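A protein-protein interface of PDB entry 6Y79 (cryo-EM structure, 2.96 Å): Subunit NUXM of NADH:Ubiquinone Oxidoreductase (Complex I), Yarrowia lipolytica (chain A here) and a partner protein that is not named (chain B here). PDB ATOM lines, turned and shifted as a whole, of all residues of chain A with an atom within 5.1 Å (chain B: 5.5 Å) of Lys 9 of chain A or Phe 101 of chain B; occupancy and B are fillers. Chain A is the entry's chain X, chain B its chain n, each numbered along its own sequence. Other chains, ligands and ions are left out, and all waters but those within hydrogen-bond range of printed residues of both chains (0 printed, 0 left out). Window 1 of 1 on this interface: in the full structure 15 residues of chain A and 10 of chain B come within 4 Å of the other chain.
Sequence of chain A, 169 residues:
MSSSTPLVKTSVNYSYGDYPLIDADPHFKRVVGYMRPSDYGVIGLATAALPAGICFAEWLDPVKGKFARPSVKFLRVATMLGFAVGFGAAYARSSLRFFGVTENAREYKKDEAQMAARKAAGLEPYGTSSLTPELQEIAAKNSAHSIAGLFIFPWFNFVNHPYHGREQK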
ATOM      1  N   LEU A   7     -28.786  12.657  -3.292  1.00  0.00           N
ATOM      2  CA  LEU A   7     -28.558  13.578  -2.160  1.00  0.00           C
ATOM      3  C   LEU A   7     -27.086  13.692  -1.724  1.00  0.00           C
ATOM      4  O   LEU A   7     -26.812  14.106  -0.592  1.00  0.00           O
ATOM      5  CB  LEU A   7     -29.468  13.245  -0.950  1.00  0.00           C
ATOM      6  CG  LEU A   7     -29.642  11.953  -0.131  1.00  0.00           C
ATOM      7  CD1 LEU A   7     -28.619  11.838   0.979  1.00  0.00           C
ATOM      8  CD2 LEU A   7     -31.042  11.893   0.453  1.00  0.00           C
ATOM      9  N   VAL A   8     -26.128  13.363  -2.613  1.00  0.00           N
ATOM     10  CA  VAL A   8     -24.705  13.600  -2.386  1.00  0.00           C
ATOM     11  C   VAL A   8     -24.076  14.176  -3.648  1.00  0.00           C
ATOM     12  O   VAL A   8     -24.644  14.125  -4.740  1.00  0.00           O
ATOM     13  CB  VAL A   8     -23.931  12.331  -1.987  1.00  0.00           C
ATOM     14  CG1 VAL A   8     -24.345  11.834  -0.614  1.00  0.00           C
ATOM     15  CG2 VAL A   8     -24.026  11.282  -3.075  1.00  0.00           C
ATOM     16  N   LYS A   9     -22.837  14.630  -3.489  1.00  0.00           N
ATOM     17  CA  LYS A   9     -22.006  15.135  -4.569  1.00  0.00           C
ATOM     18  C   LYS A   9     -21.015  14.048  -4.963  1.00  0.00           C
ATOM     19  O   LYS A   9     -20.464  13.361  -4.099  1.00  0.00           O
ATOM     20  CB  LYS A   9     -21.284  16.410  -4.134  1.00  0.00           C
ATOM     21  CG  LYS A   9     -22.227  17.507  -3.674  1.00  0.00           C
ATOM     22  CD  LYS A   9     -22.937  18.155  -4.858  1.00  0.00           C
ATOM     23  CE  LYS A   9     -24.429  17.832  -4.932  1.00  0.00           C
ATOM     24  NZ  LYS A   9     -25.037  18.355  -6.185  1.00  0.00           N
ATOM     25  N   THR A  10     -20.795  13.895  -6.263  1.00  0.00           N
ATOM     26  CA  THR A  10     -20.245  12.668  -6.819  1.00  0.00           C
ATOM     27  C   THR A  10     -19.454  13.011  -8.075  1.00  0.00           C
ATOM     28  O   THR A  10     -19.759  13.998  -8.744  1.00  0.00           O
ATOM     29  CB  THR A  10     -21.409  11.674  -7.085  1.00  0.00           C
ATOM     30  OG1 THR A  10     -21.969  11.251  -5.841  1.00  0.00           O
ATOM     31  CG2 THR A  10     -21.027  10.443  -7.881  1.00  0.00           C
ATOM     32  N   SER A  11     -18.391  12.240  -8.326  1.00  0.00           N
ATOM     33  CA  SER A  11     -17.659  12.259  -9.586  1.00  0.00           C
ATOM     34  C   SER A  11     -18.598  12.152 -10.777  1.00  0.00           C
ATOM     35  O   SER A  11     -19.587  11.413 -10.751  1.00  0.00           O
ATOM     36  CB  SER A  11     -16.697  11.094  -9.652  1.00  0.00           C
ATOM     37  OG  SER A  11     -15.844  11.066  -8.545  1.00  0.00           O
ATOM     38  N   GLU A 137     -27.381   4.752   0.115  1.00  0.00           N
ATOM     39  CA  GLU A 137     -26.130   5.497   0.114  1.00  0.00           C
ATOM     40  C   GLU A 137     -25.053   4.794   0.926  1.00  0.00           C
ATOM     41  O   GLU A 137     -23.904   4.689   0.482  1.00  0.00           O
ATOM     42  CB  GLU A 137     -26.345   6.909   0.636  1.00  0.00           C
ATOM     43  CG  GLU A 137     -25.086   7.738   0.599  1.00  0.00           C
ATOM     44  CD  GLU A 137     -25.212   9.025   1.371  1.00  0.00           C
ATOM     45  OE1 GLU A 137     -26.355   9.450   1.639  1.00  0.00           O
ATOM     46  OE2 GLU A 137     -24.168   9.606   1.725  1.00  0.00           O
ATOM     47  N   ALA A 140     -23.891   1.589  -0.878  1.00  0.00           N
ATOM     48  CA  ALA A 140     -22.986   1.840  -1.985  1.00  0.00           C
ATOM     49  C   ALA A 140     -21.692   2.504  -1.565  1.00  0.00           C
ATOM     50  O   ALA A 140     -20.747   2.512  -2.346  1.00  0.00           O
ATOM     51  CB  ALA A 140     -23.658   2.695  -3.032  1.00  0.00           C
ATOM     52  N   LYS A 141     -21.624   3.078  -0.371  1.00  0.00           N
ATOM     53  CA  LYS A 141     -20.316   3.423   0.165  1.00  0.00           C
ATOM     54  C   LYS A 141     -19.558   2.179   0.589  1.00  0.00           C
ATOM     55  O   LYS A 141     -18.324   2.186   0.606  1.00  0.00           O
ATOM     56  CB  LYS A 141     -20.448   4.378   1.341  1.00  0.00           C
ATOM     57  CG  LYS A 141     -20.692   5.800   0.949  1.00  0.00           C
ATOM     58  CD  LYS A 141     -20.823   6.661   2.173  1.00  0.00           C
ATOM     59  CE  LYS A 141     -21.178   8.080   1.813  1.00  0.00           C
ATOM     60  NZ  LYS A 141     -21.531   8.865   3.020  1.00  0.00           N
ATOM     61  N   TYR A 163     -26.565   6.200  -7.802  1.00  0.00           N
ATOM     62  CA  TYR A 163     -25.421   6.932  -8.330  1.00  0.00           C
ATOM     63  C   TYR A 163     -24.324   5.982  -8.803  1.00  0.00           C
ATOM     64  O   TYR A 163     -24.016   4.987  -8.146  1.00  0.00           O
ATOM     65  CB  TYR A 163     -24.883   7.924  -7.293  1.00  0.00           C
ATOM     66  CG  TYR A 163     -24.695   7.354  -5.922  1.00  0.00           C
ATOM     67  CD1 TYR A 163     -23.559   6.644  -5.623  1.00  0.00           C
ATOM     68  CD2 TYR A 163     -25.639   7.553  -4.920  1.00  0.00           C
ATOM     69  CE1 TYR A 163     -23.378   6.105  -4.426  1.00  0.00           C
ATOM     70  CE2 TYR A 163     -25.454   7.027  -3.681  1.00  0.00           C
ATOM     71  CZ  TYR A 163     -24.310   6.303  -3.448  1.00  0.00           C
ATOM     72  OH  TYR A 163     -24.033   5.760  -2.236  1.00  0.00           O
ATOM     73  N   TYR B  93      -8.373  15.801  -3.522  1.00  0.00           N
ATOM     74  CA  TYR B  93      -9.075  14.843  -2.677  1.00  0.00           C
ATOM     75  C   TYR B  93      -9.639  13.690  -3.490  1.00  0.00           C
ATOM     76  O   TYR B  93      -9.750  12.573  -2.979  1.00  0.00           O
ATOM     77  CB  TYR B  93     -10.184  15.562  -1.919  1.00  0.00           C
ATOM     78  CG  TYR B  93     -11.004  14.730  -0.961  1.00  0.00           C
ATOM     79  CD1 TYR B  93     -10.577  14.499   0.334  1.00  0.00           C
ATOM     80  CD2 TYR B  93     -12.232  14.213  -1.345  1.00  0.00           C
ATOM     81  CE1 TYR B  93     -11.337  13.763   1.206  1.00  0.00           C
ATOM     82  CE2 TYR B  93     -12.996  13.477  -0.478  1.00  0.00           C
ATOM     83  CZ  TYR B  93     -12.547  13.262   0.798  1.00  0.00           C
ATOM     84  OH  TYR B  93     -13.308  12.518   1.667  1.00  0.00           O
ATOM     85  N   TYR B  97      -7.903  10.517  -1.880  1.00  0.00           N
ATOM     86  CA  TYR B  97      -8.924   9.683  -1.271  1.00  0.00           C
ATOM     87  C   TYR B  97      -9.689   9.045  -2.437  1.00  0.00           C
ATOM     88  O   TYR B  97      -9.297   9.211  -3.591  1.00  0.00           O
ATOM     89  CB  TYR B  97      -9.716  10.552  -0.280  1.00  0.00           C
ATOM     90  CG  TYR B  97     -10.926   9.943   0.398  1.00  0.00           C
ATOM     91  CD1 TYR B  97     -10.806   9.221   1.573  1.00  0.00           C
ATOM     92  CD2 TYR B  97     -12.199  10.104  -0.151  1.00  0.00           C
ATOM     93  CE1 TYR B  97     -11.919   8.663   2.174  1.00  0.00           C
ATOM     94  CE2 TYR B  97     -13.303   9.547   0.424  1.00  0.00           C
ATOM     95  CZ  TYR B  97     -13.169   8.832   1.585  1.00  0.00           C
ATOM     96  OH  TYR B  97     -14.296   8.290   2.159  1.00  0.00           O
ATOM     97  N   SER B  98     -10.739   8.275  -2.159  1.00  0.00           N
ATOM     98  CA  SER B  98     -11.557   7.624  -3.175  1.00  0.00           C
ATOM     99  C   SER B  98     -12.165   8.626  -4.158  1.00  0.00           C
ATOM    100  O   SER B  98     -12.577   9.722  -3.752  1.00  0.00           O
ATOM    101  CB  SER B  98     -12.687   6.824  -2.522  1.00  0.00           C
ATOM    102  OG  SER B  98     -13.519   6.208  -3.487  1.00  0.00           O
ATOM    103  N   PRO B  99     -12.228   8.285  -5.439  1.00  0.00           N
ATOM    104  CA  PRO B  99     -12.738   9.184  -6.476  1.00  0.00           C
ATOM    105  C   PRO B  99     -14.220   9.479  -6.412  1.00  0.00           C
ATOM    106  O   PRO B  99     -14.625  10.644  -6.414  1.00  0.00           O
ATOM    107  CB  PRO B  99     -12.420   8.406  -7.749  1.00  0.00           C
ATOM    108  CG  PRO B  99     -11.309   7.541  -7.364  1.00  0.00           C
ATOM    109  CD  PRO B  99     -11.640   7.082  -6.032  1.00  0.00           C
ATOM    110  N   LEU B 100     -15.025   8.419  -6.425  1.00  0.00           N
ATOM    111  CA  LEU B 100     -16.433   8.515  -6.070  1.00  0.00           C
ATOM    112  C   LEU B 100     -16.538   9.049  -4.654  1.00  0.00           C
ATOM    113  O   LEU B 100     -15.712   8.709  -3.800  1.00  0.00           O
ATOM    114  CB  LEU B 100     -17.075   7.134  -6.173  1.00  0.00           C
ATOM    115  CG  LEU B 100     -18.566   6.828  -6.202  1.00  0.00           C
ATOM    116  CD1 LEU B 100     -19.139   7.339  -7.465  1.00  0.00           C
ATOM    117  CD2 LEU B 100     -18.779   5.337  -6.121  1.00  0.00           C
ATOM    118  N   PHE B 101     -17.550   9.891  -4.419  1.00  0.00           N
ATOM    119  CA  PHE B 101     -17.726  10.679  -3.195  1.00  0.00           C
ATOM    120  C   PHE B 101     -16.538  11.616  -2.968  1.00  0.00           C
ATOM    121  O   PHE B 101     -15.775  11.496  -2.011  1.00  0.00           O
ATOM    122  CB  PHE B 101     -17.954   9.797  -1.963  1.00  0.00           C
ATOM    123  CG  PHE B 101     -19.217   9.058  -2.000  1.00  0.00           C
ATOM    124  CD1 PHE B 101     -20.379   9.674  -1.586  1.00  0.00           C
ATOM    125  CD2 PHE B 101     -19.264   7.757  -2.458  1.00  0.00           C
ATOM    126  CE1 PHE B 101     -21.563   9.011  -1.617  1.00  0.00           C
ATOM    127  CE2 PHE B 101     -20.449   7.088  -2.492  1.00  0.00           C
ATOM    128  CZ  PHE B 101     -21.591   7.718  -2.055  1.00  0.00           C
ATOM    129  N   SER B 102     -16.422  12.571  -3.883  1.00  0.00           N
ATOM    130  CA  SER B 102     -15.336  13.536  -3.851  1.00  0.00           C
ATOM    131  C   SER B 102     -15.558  14.683  -2.871  1.00  0.00           C
ATOM    132  O   SER B 102     -14.714  15.584  -2.824  1.00  0.00           O
ATOM    133  CB  SER B 102     -15.109  14.105  -5.249  1.00  0.00           C
ATOM    134  OG  SER B 102     -14.671  13.098  -6.135  1.00  0.00           O
ATOM    135  N   ASP B 103     -16.743  14.698  -2.050  1.00  0.00           N
ATOM    136  CA  ASP B 103     -16.618  15.848  -1.167  1.00  0.00           C
ATOM    137  C   ASP B 103     -16.287  15.417   0.258  1.00  0.00           C
ATOM    138  O   ASP B 103     -16.786  14.398   0.743  1.00  0.00           O
ATOM    139  CB  ASP B 103     -17.890  16.700  -1.181  1.00  0.00           C
ATOM    140  CG  ASP B 103     -19.118  15.965  -0.690  1.00  0.00           C
ATOM    141  OD1 ASP B 103     -19.182  14.724  -0.808  1.00  0.00           O
ATOM    142  OD2 ASP B 103     -20.026  16.649  -0.172  1.00  0.00           O
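The side-chain carboxylate (OE2) of Glu 137 of chain A lies within salt-bridge range of the side-chain amino group (NZ) of Lys 141 of chain A (3.0 Å).
The backbone carbonyl oxygen (O) of Glu 137 of chain A lies within hydrogen-bond range of the side-chain hydroxyl (OH) of Tyr 163 of chain A (2.9 Å).
OG of Ser 98 of chain B is in hydrogen-bond range of O of Leu 100 of chain B, 3.3 Å away.
The backbone carbonyl oxygen (O) of Pro 99 of chain B lies within hydrogen-bond range of the side-chain hydroxyl (OG) of Ser 102 of chain B (2.5 Å).
Among the printed residues, pairs that only touch across the chains: Val 8 of chain A with Phe 101 of chain B, Lys 9 of chain A with Phe 101 of chain B, Lys 9 of chain A with Asp 103 of chain B, Thr 10 of chain A with Leu 100 of chain B, Lys 141 of chain A with Phe 101 of chain B and Tyr 163 of chain A with Phe 101 of chain B.
O of Pro 99 of chain B lies within hydrogen-bond range of OG of Ser 11 of chain A (2.5 Å).
The side-chain hydroxyl (OG) of Ser 11 of chain A sits at hydrogen-bond distance from the backbone NH (N) of Leu 100 of chain B.
OG of Ser 11 of chain A lies within hydrogen-bond range of OG of Ser 102 of chain B.
Lys 9 of chain A touches just these residues of chain B: Phe 101 (3.9 Å) and Asp 103 (3.8 Å).
Of the printed residues of chain A, Phe 101 of chain B touches Val 8, Lys 9, Lys 141 and Tyr 163.
Of the printed residues of chain A, Asp 103 of chain B touches Lys 9.
Of the printed residues of chain B, Tyr 163 of chain A touches Phe 101.
Of the printed residues of chain B, Val 8 of chain A touches Phe 101 (3.7 Å).
Of the printed residues of chain B, Lys 141 of chain A touches Phe 101.
Tyr 97 of chain B touches none of the printed residues of chain A.
Leu 7 of chain A touches none of the printed residues of chain B.
The nearest residue of chain B that does not touch Lys 9 of chain A is Ser 102 of chain B (4.1 Å).
Hydrophobic or aromatic side chains of chain A within 4 Å of the printed part of chain B: Val 8 and Tyr 163.
Of the 8 printed residues of chain B, 5 touch a printed residue of chain A.
Printed residues of chain B that touch a printed residue of chain A: Pro 99, Leu 100, Phe 101, Ser 102 and Asp 103.
Hydrophobic or aromatic side chains of chain B within 4 Å of the printed part of chain A: Leu 100 and Phe 101.
Among the printed residues, 9 pairs touch across the chains.
Among the printed residues, no Asp or Glu carboxylate lies within 4 Å of a Lys or Arg side-chain nitrogen of the other chain.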
